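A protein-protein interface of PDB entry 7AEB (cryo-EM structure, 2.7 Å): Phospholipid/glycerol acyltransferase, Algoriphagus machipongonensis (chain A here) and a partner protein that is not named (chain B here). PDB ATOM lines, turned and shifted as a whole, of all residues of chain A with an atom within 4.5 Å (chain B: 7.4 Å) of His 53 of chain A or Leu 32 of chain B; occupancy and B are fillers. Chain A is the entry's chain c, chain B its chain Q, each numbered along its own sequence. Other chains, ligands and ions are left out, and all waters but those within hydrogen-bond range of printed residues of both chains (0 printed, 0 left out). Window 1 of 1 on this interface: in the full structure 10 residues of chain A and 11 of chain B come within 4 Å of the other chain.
OE2 of Glu 45 of chain A is in hydrogen-bond range of N of Asn 33 of chain B (3.2 Å).
The backbone carbonyl oxygen of Leu 32 of chain B sits at hydrogen-bond distance from the side-chain hydroxyl of Thr 30 of chain B (3.0 Å).
The backbone carbonyl oxygen (O) of Phe 43 of chain A sits at hydrogen-bond distance from the backbone NH (N) of His 53 of chain A (2.9 Å).
NZ of Lys 8 of chain B lies within hydrogen-bond range of OH of Tyr 83 of chain B (3.4 Å).
N of Glu 41 of chain A is in hydrogen-bond range of O of Phe 55 of chain A, 2.8 Å away.
N of Leu 9 of chain B sits at hydrogen-bond distance from OD1 of Asn 33 of chain B (3.2 Å).
The side-chain carboxylate of Glu 45 of chain A sits at hydrogen-bond distance from a ring nitrogen (NE2) of His 53 of chain A.
Among the printed residues, merely in contact across the chains: Phe 43 of chain A with Asn 33 of chain B, Glu 45 of chain A with Lys 8 of chain B, Glu 45 of chain A with Leu 32 of chain B, His 53 of chain A with Leu 32 of chain B, Lys 54 of chain A with Val 79 of chain B, Phe 55 of chain A with Asp 75 of chain B and Phe 55 of chain A with Ile 80 of chain B.
Of the printed residues of chain B, His 53 of chain A touches Leu 32 (3.99 Å).
Of the printed residues of chain B, Lys 54 of chain A touches Val 79 (3.9 Å).
Of the printed residues of chain A, Leu 32 of chain B touches Glu 45 (3.6 Å) and His 53 (3.99 Å).
Glu 35 of chain B touches none of the printed residues of chain A.
Phe 72 of chain B touches none of the printed residues of chain A.
Printed residues of chain A within 4 Å of Val 79 of chain B: Lys 54.
The nearest printed residue of chain A that does not touch Ile 80 of chain B is His 53 of chain A (4.6 Å).
Printed residues of chain B that touch a printed residue of chain A: Lys 8, Leu 32, Asn 33, Asp 75, Val 79 and Ile 80.
Printed residues of chain A that touch a printed residue of chain B: Phe 43, Glu 45, His 53, Lys 54 and Phe 55.
Hydrophobic or aromatic side chains of chain A that line the printed part of chain B: Phe 43, His 53 and Phe 55.
Among the printed residues, no Asp or Glu carboxylate lies within 4 Å of a Lys or Arg side-chain nitrogen of the other chain.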
ATOM      1  N   GLU A  41       7.789  -9.335  16.490  1.00  0.00           N
ATOM      2  CA  GLU A  41       8.701 -10.481  16.551  1.00  0.00           C
ATOM      3  C   GLU A  41      10.131 -10.102  16.858  1.00  0.00           C
ATOM      4  O   GLU A  41      10.570  -9.013  16.519  1.00  0.00           O
ATOM      5  CB  GLU A  41       8.696 -11.350  15.301  1.00  0.00           C
ATOM      6  CG  GLU A  41       7.394 -11.938  14.936  1.00  0.00           C
ATOM      7  CD  GLU A  41       7.460 -12.687  13.640  1.00  0.00           C
ATOM      8  OE1 GLU A  41       8.460 -12.548  12.938  1.00  0.00           O
ATOM      9  OE2 GLU A  41       6.515 -13.413  13.315  1.00  0.00           O
ATOM     10  N   GLU A  42      10.869 -11.017  17.486  1.00  0.00           N
ATOM     11  CA  GLU A  42      12.252 -10.745  17.856  1.00  0.00           C
ATOM     12  C   GLU A  42      13.267 -11.537  17.033  1.00  0.00           C
ATOM     13  O   GLU A  42      12.997 -12.654  16.590  1.00  0.00           O
ATOM     14  CB  GLU A  42      12.474 -11.066  19.326  1.00  0.00           C
ATOM     15  CG  GLU A  42      11.793 -10.108  20.269  1.00  0.00           C
ATOM     16  CD  GLU A  42      11.991 -10.458  21.728  1.00  0.00           C
ATOM     17  OE1 GLU A  42      12.866 -11.272  22.051  1.00  0.00           O
ATOM     18  OE2 GLU A  42      11.449  -9.726  22.569  1.00  0.00           O
ATOM     19  N   PHE A  43      14.471 -10.962  16.889  1.00  0.00           N
ATOM     20  CA  PHE A  43      15.581 -11.616  16.201  1.00  0.00           C
ATOM     21  C   PHE A  43      16.949 -11.258  16.788  1.00  0.00           C
ATOM     22  O   PHE A  43      17.256 -10.087  17.018  1.00  0.00           O
ATOM     23  CB  PHE A  43      15.556 -11.251  14.726  1.00  0.00           C
ATOM     24  CG  PHE A  43      16.693 -11.792  13.964  1.00  0.00           C
ATOM     25  CD1 PHE A  43      16.728 -13.113  13.588  1.00  0.00           C
ATOM     26  CD2 PHE A  43      17.735 -10.968  13.606  1.00  0.00           C
ATOM     27  CE1 PHE A  43      17.797 -13.599  12.881  1.00  0.00           C
ATOM     28  CE2 PHE A  43      18.795 -11.446  12.911  1.00  0.00           C
ATOM     29  CZ  PHE A  43      18.830 -12.763  12.546  1.00  0.00           C
ATOM     30  N   GLU A  45      20.894 -11.020  16.129  1.00  0.00           N
ATOM     31  CA  GLU A  45      21.899 -10.945  15.082  1.00  0.00           C
ATOM     32  C   GLU A  45      23.263 -11.296  15.656  1.00  0.00           C
ATOM     33  O   GLU A  45      23.681 -10.699  16.647  1.00  0.00           O
ATOM     34  CB  GLU A  45      21.926  -9.542  14.488  1.00  0.00           C
ATOM     35  CG  GLU A  45      22.899  -9.392  13.373  1.00  0.00           C
ATOM     36  CD  GLU A  45      22.937  -8.020  12.804  1.00  0.00           C
ATOM     37  OE1 GLU A  45      22.265  -7.121  13.322  1.00  0.00           O
ATOM     38  OE2 GLU A  45      23.640  -7.833  11.816  1.00  0.00           O
ATOM     39  N   PHE A  51      21.493  -5.550  22.082  1.00  0.00           N
ATOM     40  CA  PHE A  51      20.035  -5.644  22.067  1.00  0.00           C
ATOM     41  C   PHE A  51      19.593  -6.658  21.018  1.00  0.00           C
ATOM     42  O   PHE A  51      20.352  -7.015  20.119  1.00  0.00           O
ATOM     43  CB  PHE A  51      19.379  -4.285  21.788  1.00  0.00           C
ATOM     44  CG  PHE A  51      19.877  -3.603  20.557  1.00  0.00           C
ATOM     45  CD1 PHE A  51      19.295  -3.846  19.334  1.00  0.00           C
ATOM     46  CD2 PHE A  51      20.911  -2.702  20.627  1.00  0.00           C
ATOM     47  CE1 PHE A  51      19.751  -3.239  18.219  1.00  0.00           C
ATOM     48  CE2 PHE A  51      21.370  -2.089  19.507  1.00  0.00           C
ATOM     49  CZ  PHE A  51      20.790  -2.355  18.303  1.00  0.00           C
ATOM     50  N   LYS A  52      18.335  -7.068  21.100  1.00  0.00           N
ATOM     51  CA  LYS A  52      17.746  -7.861  20.031  1.00  0.00           C
ATOM     52  C   LYS A  52      16.935  -6.941  19.142  1.00  0.00           C
ATOM     53  O   LYS A  52      16.499  -5.879  19.569  1.00  0.00           O
ATOM     54  CB  LYS A  52      16.857  -8.972  20.579  1.00  0.00           C
ATOM     55  CG  LYS A  52      17.588 -10.001  21.390  1.00  0.00           C
ATOM     56  CD  LYS A  52      16.633 -11.011  21.995  1.00  0.00           C
ATOM     57  CE  LYS A  52      16.126 -12.024  20.978  1.00  0.00           C
ATOM     58  NZ  LYS A  52      15.162 -12.973  21.597  1.00  0.00           N
ATOM     59  N   HIS A  53      16.737  -7.351  17.899  1.00  0.00           N
ATOM     60  CA  HIS A  53      15.937  -6.561  16.982  1.00  0.00           C
ATOM     61  C   HIS A  53      14.472  -6.900  17.165  1.00  0.00           C
ATOM     62  O   HIS A  53      14.126  -8.031  17.493  1.00  0.00           O
ATOM     63  CB  HIS A  53      16.325  -6.845  15.544  1.00  0.00           C
ATOM     64  CG  HIS A  53      17.717  -6.454  15.203  1.00  0.00           C
ATOM     65  ND1 HIS A  53      18.119  -5.142  15.094  1.00  0.00           N
ATOM     66  CD2 HIS A  53      18.804  -7.206  14.924  1.00  0.00           C
ATOM     67  CE1 HIS A  53      19.395  -5.104  14.762  1.00  0.00           C
ATOM     68  NE2 HIS A  53      19.831  -6.344  14.649  1.00  0.00           N
ATOM     69  N   LYS A  54      13.607  -5.926  16.924  1.00  0.00           N
ATOM     70  CA  LYS A  54      12.174  -6.150  17.011  1.00  0.00           C
ATOM     71  C   LYS A  54      11.501  -5.657  15.747  1.00  0.00           C
ATOM     72  O   LYS A  54      11.830  -4.586  15.246  1.00  0.00           O
ATOM     73  CB  LYS A  54      11.587  -5.437  18.214  1.00  0.00           C
ATOM     74  CG  LYS A  54      12.170  -5.924  19.493  1.00  0.00           C
ATOM     75  CD  LYS A  54      11.583  -5.263  20.688  1.00  0.00           C
ATOM     76  CE  LYS A  54      12.270  -5.773  21.944  1.00  0.00           C
ATOM     77  NZ  LYS A  54      11.738  -5.130  23.174  1.00  0.00           N
ATOM     78  N   PHE A  55      10.534  -6.417  15.259  1.00  0.00           N
ATOM     79  CA  PHE A  55       9.860  -6.063  14.027  1.00  0.00           C
ATOM     80  C   PHE A  55       8.360  -6.101  14.221  1.00  0.00           C
ATOM     81  O   PHE A  55       7.881  -7.015  14.840  1.00  0.00           O
ATOM     82  CB  PHE A  55      10.204  -7.049  12.935  1.00  0.00           C
ATOM     83  CG  PHE A  55      11.631  -7.211  12.751  1.00  0.00           C
ATOM     84  CD1 PHE A  55      12.284  -8.204  13.421  1.00  0.00           C
ATOM     85  CD2 PHE A  55      12.343  -6.372  11.930  1.00  0.00           C
ATOM     86  CE1 PHE A  55      13.611  -8.367  13.292  1.00  0.00           C
ATOM     87  CE2 PHE A  55      13.693  -6.539  11.788  1.00  0.00           C
ATOM     88  CZ  PHE A  55      14.325  -7.541  12.474  1.00  0.00           C
ATOM     89  N   LEU B   6      31.255  -3.633  13.296  1.00  0.00           N
ATOM     90  CA  LEU B   6      30.469  -4.854  13.144  1.00  0.00           C
ATOM     91  C   LEU B   6      30.661  -5.388  11.731  1.00  0.00           C
ATOM     92  O   LEU B   6      30.153  -4.814  10.764  1.00  0.00           O
ATOM     93  CB  LEU B   6      28.995  -4.585  13.434  1.00  0.00           C
ATOM     94  CG  LEU B   6      28.048  -5.791  13.410  1.00  0.00           C
ATOM     95  CD1 LEU B   6      28.376  -6.766  14.512  1.00  0.00           C
ATOM     96  CD2 LEU B   6      26.606  -5.356  13.519  1.00  0.00           C
ATOM     97  N   LYS B   8      30.169  -7.875   8.529  1.00  0.00           N
ATOM     98  CA  LYS B   8      29.042  -8.552   7.907  1.00  0.00           C
ATOM     99  C   LYS B   8      29.532  -9.701   7.035  1.00  0.00           C
ATOM    100  O   LYS B   8      30.604  -9.620   6.433  1.00  0.00           O
ATOM    101  CB  LYS B   8      28.226  -7.566   7.076  1.00  0.00           C
ATOM    102  CG  LYS B   8      27.423  -6.599   7.912  1.00  0.00           C
ATOM    103  CD  LYS B   8      26.227  -7.288   8.525  1.00  0.00           C
ATOM    104  CE  LYS B   8      25.699  -6.521   9.705  1.00  0.00           C
ATOM    105  NZ  LYS B   8      25.387  -5.120   9.351  1.00  0.00           N
ATOM    106  N   LEU B   9      28.739 -10.766   6.968  1.00  0.00           N
ATOM    107  CA  LEU B   9      29.122 -11.979   6.254  1.00  0.00           C
ATOM    108  C   LEU B   9      29.052 -11.764   4.741  1.00  0.00           C
ATOM    109  O   LEU B   9      28.175 -11.061   4.241  1.00  0.00           O
ATOM    110  CB  LEU B   9      28.217 -13.128   6.706  1.00  0.00           C
ATOM    111  CG  LEU B   9      28.022 -14.465   5.984  1.00  0.00           C
ATOM    112  CD1 LEU B   9      29.312 -15.162   5.754  1.00  0.00           C
ATOM    113  CD2 LEU B   9      27.146 -15.359   6.804  1.00  0.00           C
ATOM    114  N   PHE B  28      28.011 -11.315  -2.854  1.00  0.00           N
ATOM    115  CA  PHE B  28      26.850 -11.028  -2.026  1.00  0.00           C
ATOM    116  C   PHE B  28      27.309 -10.614  -0.636  1.00  0.00           C
ATOM    117  O   PHE B  28      28.203 -11.239  -0.061  1.00  0.00           O
ATOM    118  CB  PHE B  28      25.929 -12.255  -1.950  1.00  0.00           C
ATOM    119  CG  PHE B  28      24.809 -12.118  -0.957  1.00  0.00           C
ATOM    120  CD1 PHE B  28      23.701 -11.352  -1.255  1.00  0.00           C
ATOM    121  CD2 PHE B  28      24.861 -12.767   0.268  1.00  0.00           C
ATOM    122  CE1 PHE B  28      22.671 -11.223  -0.349  1.00  0.00           C
ATOM    123  CE2 PHE B  28      23.837 -12.633   1.176  1.00  0.00           C
ATOM    124  CZ  PHE B  28      22.738 -11.865   0.864  1.00  0.00           C
ATOM    125  N   ILE B  29      26.708  -9.556  -0.100  1.00  0.00           N
ATOM    126  CA  ILE B  29      26.943  -9.109   1.267  1.00  0.00           C
ATOM    127  C   ILE B  29      25.596  -9.042   1.968  1.00  0.00           C
ATOM    128  O   ILE B  29      24.659  -8.428   1.455  1.00  0.00           O
ATOM    129  CB  ILE B  29      27.653  -7.741   1.320  1.00  0.00           C
ATOM    130  CG1 ILE B  29      28.929  -7.752   0.482  1.00  0.00           C
ATOM    131  CG2 ILE B  29      27.994  -7.364   2.743  1.00  0.00           C
ATOM    132  CD1 ILE B  29      29.451  -6.392   0.147  1.00  0.00           C
ATOM    133  N   THR B  30      25.500  -9.665   3.136  1.00  0.00           N
ATOM    134  CA  THR B  30      24.250  -9.673   3.877  1.00  0.00           C
ATOM    135  C   THR B  30      24.047  -8.349   4.617  1.00  0.00           C
ATOM    136  O   THR B  30      24.975  -7.560   4.812  1.00  0.00           O
ATOM    137  CB  THR B  30      24.209 -10.855   4.847  1.00  0.00           C
ATOM    138  OG1 THR B  30      22.858 -11.112   5.237  1.00  0.00           O
ATOM    139  CG2 THR B  30      25.026 -10.580   6.094  1.00  0.00           C
ATOM    140  N   LEU B  31      22.803  -8.094   5.003  1.00  0.00           N
ATOM    141  CA  LEU B  31      22.488  -6.924   5.811  1.00  0.00           C
ATOM    142  C   LEU B  31      22.255  -7.263   7.275  1.00  0.00           C
ATOM    143  O   LEU B  31      22.355  -6.375   8.124  1.00  0.00           O
ATOM    144  CB  LEU B  31      21.256  -6.201   5.259  1.00  0.00           C
ATOM    145  CG  LEU B  31      21.308  -5.711   3.806  1.00  0.00           C
ATOM    146  CD1 LEU B  31      19.911  -5.592   3.252  1.00  0.00           C
ATOM    147  CD2 LEU B  31      22.033  -4.389   3.674  1.00  0.00           C
ATOM    148  N   LEU B  32      21.929  -8.516   7.582  1.00  0.00           N
ATOM    149  CA  LEU B  32      21.843  -9.005   8.949  1.00  0.00           C
ATOM    150  C   LEU B  32      22.564 -10.337   9.041  1.00  0.00           C
ATOM    151  O   LEU B  32      22.346 -11.226   8.219  1.00  0.00           O
ATOM    152  CB  LEU B  32      20.394  -9.166   9.406  1.00  0.00           C
ATOM    153  CG  LEU B  32      19.525  -7.912   9.453  1.00  0.00           C
ATOM    154  CD1 LEU B  32      18.070  -8.293   9.304  1.00  0.00           C
ATOM    155  CD2 LEU B  32      19.757  -7.147  10.738  1.00  0.00           C
ATOM    156  N   ASN B  33      23.408 -10.459  10.030  1.00  0.00           N
ATOM    157  CA  ASN B  33      24.211 -11.640  10.294  1.00  0.00           C
ATOM    158  C   ASN B  33      23.348 -12.773  10.841  1.00  0.00           C
ATOM    159  O   ASN B  33      22.345 -12.524  11.512  1.00  0.00           O
ATOM    160  CB  ASN B  33      25.302 -11.310  11.313  1.00  0.00           C
ATOM    161  CG  ASN B  33      26.544 -10.743  10.674  1.00  0.00           C
ATOM    162  OD1 ASN B  33      26.989 -11.226   9.648  1.00  0.00           O
ATOM    163  ND2 ASN B  33      27.104  -9.711  11.278  1.00  0.00           N
ATOM    164  N   PRO B  34      23.717 -14.024  10.574  1.00  0.00           N
ATOM    165  CA  PRO B  34      23.067 -15.143  11.262  1.00  0.00           C
ATOM    166  C   PRO B  34      23.387 -15.129  12.751  1.00  0.00           C
ATOM    167  O   PRO B  34      24.322 -14.472  13.206  1.00  0.00           O
ATOM    168  CB  PRO B  34      23.658 -16.378  10.574  1.00  0.00           C
ATOM    169  CG  PRO B  34      24.211 -15.891   9.301  1.00  0.00           C
ATOM    170  CD  PRO B  34      24.646 -14.491   9.534  1.00  0.00           C
ATOM    171  N   GLU B  35      22.523 -15.790  13.517  1.00  0.00           N
ATOM    172  CA  GLU B  35      22.720 -15.981  14.957  1.00  0.00           C
ATOM    173  C   GLU B  35      23.851 -16.936  15.327  1.00  0.00           C
ATOM    174  O   GLU B  35      24.581 -16.704  16.300  1.00  0.00           O
ATOM    175  CB  GLU B  35      21.410 -16.430  15.605  1.00  0.00           C
ATOM    176  CG  GLU B  35      21.496 -16.615  17.110  1.00  0.00           C
ATOM    177  CD  GLU B  35      20.212 -17.142  17.712  1.00  0.00           C
ATOM    178  OE1 GLU B  35      19.211 -17.250  16.971  1.00  0.00           O
ATOM    179  OE2 GLU B  35      20.173 -17.362  18.940  1.00  0.00           O
ATOM    180  N   ASP B  71      21.126 -19.797   8.869  1.00  0.00           N
ATOM    181  CA  ASP B  71      19.863 -19.179   8.461  1.00  0.00           C
ATOM    182  C   ASP B  71      19.992 -17.677   8.217  1.00  0.00           C
ATOM    183  O   ASP B  71      20.774 -17.017   8.865  1.00  0.00           O
ATOM    184  CB  ASP B  71      18.821 -19.378   9.538  1.00  0.00           C
ATOM    185  CG  ASP B  71      18.230 -20.752   9.530  1.00  0.00           C
ATOM    186  OD1 ASP B  71      17.450 -21.023   8.655  1.00  0.00           O
ATOM    187  OD2 ASP B  71      18.512 -21.564  10.423  1.00  0.00           O
ATOM    188  N   PHE B  72      19.192 -17.125   7.310  1.00  0.00           N
ATOM    189  CA  PHE B  72      19.238 -15.708   6.955  1.00  0.00           C
ATOM    190  C   PHE B  72      17.891 -15.041   7.097  1.00  0.00           C
ATOM    191  O   PHE B  72      16.876 -15.674   6.976  1.00  0.00           O
ATOM    192  CB  PHE B  72      19.591 -15.512   5.490  1.00  0.00           C
ATOM    193  CG  PHE B  72      21.034 -15.489   5.207  1.00  0.00           C
ATOM    194  CD1 PHE B  72      21.530 -16.167   4.135  1.00  0.00           C
ATOM    195  CD2 PHE B  72      21.899 -14.796   6.010  1.00  0.00           C
ATOM    196  CE1 PHE B  72      22.876 -16.151   3.859  1.00  0.00           C
ATOM    197  CE2 PHE B  72      23.249 -14.770   5.746  1.00  0.00           C
ATOM    198  CZ  PHE B  72      23.741 -15.448   4.663  1.00  0.00           C
ATOM    199  N   LEU B  73      17.891 -13.736   7.286  1.00  0.00           N
ATOM    200  CA  LEU B  73      16.669 -12.945   7.331  1.00  0.00           C
ATOM    201  C   LEU B  73      16.826 -11.720   6.442  1.00  0.00           C
ATOM    202  O   LEU B  73      17.838 -11.018   6.521  1.00  0.00           O
ATOM    203  CB  LEU B  73      16.336 -12.523   8.762  1.00  0.00           C
ATOM    204  CG  LEU B  73      15.095 -11.654   8.962  1.00  0.00           C
ATOM    205  CD1 LEU B  73      13.840 -12.487   8.891  1.00  0.00           C
ATOM    206  CD2 LEU B  73      15.167 -10.914  10.272  1.00  0.00           C
ATOM    207  N   PHE B  74      15.834 -11.482   5.589  1.00  0.00           N
ATOM    208  CA  PHE B  74      15.768 -10.332   4.695  1.00  0.00           C
ATOM    209  C   PHE B  74      14.602  -9.460   5.137  1.00  0.00           C
ATOM    210  O   PHE B  74      13.481  -9.955   5.253  1.00  0.00           O
ATOM    211  CB  PHE B  74      15.541 -10.755   3.236  1.00  0.00           C
ATOM    212  CG  PHE B  74      16.629 -11.614   2.642  1.00  0.00           C
ATOM    213  CD1 PHE B  74      16.692 -12.975   2.902  1.00  0.00           C
ATOM    214  CD2 PHE B  74      17.551 -11.067   1.767  1.00  0.00           C
ATOM    215  CE1 PHE B  74      17.677 -13.758   2.340  1.00  0.00           C
ATOM    216  CE2 PHE B  74      18.535 -11.851   1.198  1.00  0.00           C
ATOM    217  CZ  PHE B  74      18.599 -13.196   1.487  1.00  0.00           C
ATOM    218  N   ASP B  75      14.846  -8.171   5.363  1.00  0.00           N
ATOM    219  CA  ASP B  75      13.766  -7.290   5.805  1.00  0.00           C
ATOM    220  C   ASP B  75      14.053  -5.858   5.384  1.00  0.00           C
ATOM    221  O   ASP B  75      15.134  -5.337   5.665  1.00  0.00           O
ATOM    222  CB  ASP B  75      13.580  -7.374   7.323  1.00  0.00           C
ATOM    223  CG  ASP B  75      12.496  -6.445   7.831  1.00  0.00           C
ATOM    224  OD1 ASP B  75      12.828  -5.368   8.359  1.00  0.00           O
ATOM    225  OD2 ASP B  75      11.308  -6.791   7.705  1.00  0.00           O
ATOM    226  N   VAL B  79      12.780  -0.197  10.210  1.00  0.00           N
ATOM    227  CA  VAL B  79      13.022   0.009  11.631  1.00  0.00           C
ATOM    228  C   VAL B  79      14.458  -0.304  12.020  1.00  0.00           C
ATOM    229  O   VAL B  79      14.818  -0.170  13.194  1.00  0.00           O
ATOM    230  CB  VAL B  79      12.039  -0.806  12.492  1.00  0.00           C
ATOM    231  CG1 VAL B  79      10.617  -0.293  12.315  1.00  0.00           C
ATOM    232  CG2 VAL B  79      12.130  -2.280  12.154  1.00  0.00           C
ATOM    233  N   ILE B  80      15.292  -0.707  11.071  1.00  0.00           N
ATOM    234  CA  ILE B  80      16.676  -1.074  11.333  1.00  0.00           C
ATOM    235  C   ILE B  80      17.552   0.098  10.923  1.00  0.00           C
ATOM    236  O   ILE B  80      17.486   0.564   9.780  1.00  0.00           O
ATOM    237  CB  ILE B  80      17.066  -2.362  10.592  1.00  0.00           C
ATOM    238  CG1 ILE B  80      16.255  -3.533  11.147  1.00  0.00           C
ATOM    239  CG2 ILE B  80      18.555  -2.616  10.699  1.00  0.00           C
ATOM    240  CD1 ILE B  80      16.708  -4.887  10.679  1.00  0.00           C
ATOM    241  N   ALA B  81      18.371   0.576  11.858  1.00  0.00           N
ATOM    242  CA  ALA B  81      19.153   1.785  11.644  1.00  0.00           C
ATOM    243  C   ALA B  81      20.284   1.546  10.651  1.00  0.00           C
ATOM    244  O   ALA B  81      20.998   0.545  10.727  1.00  0.00           O
ATOM    245  CB  ALA B  81      19.721   2.284  12.971  1.00  0.00           C
ATOM    246  N   TYR B  83      19.779   1.665   7.117  1.00  0.00           N
ATOM    247  CA  TYR B  83      19.299   1.246   5.813  1.00  0.00           C
ATOM    248  C   TYR B  83      18.065   2.043   5.420  1.00  0.00           C
ATOM    249  O   TYR B  83      17.413   2.668   6.259  1.00  0.00           O
ATOM    250  CB  TYR B  83      18.983  -0.249   5.800  1.00  0.00           C
ATOM    251  CG  TYR B  83      20.178  -1.085   6.153  1.00  0.00           C
ATOM    252  CD1 TYR B  83      21.406  -0.838   5.561  1.00  0.00           C
ATOM    253  CD2 TYR B  83      20.092  -2.104   7.092  1.00  0.00           C
ATOM    254  CE1 TYR B  83      22.521  -1.586   5.884  1.00  0.00           C
ATOM    255  CE2 TYR B  83      21.200  -2.866   7.422  1.00  0.00           C
ATOM    256  CZ  TYR B  83      22.413  -2.601   6.812  1.00  0.00           C
ATOM    257  OH  TYR B  83      23.526  -3.345   7.126  1.00  0.00           O
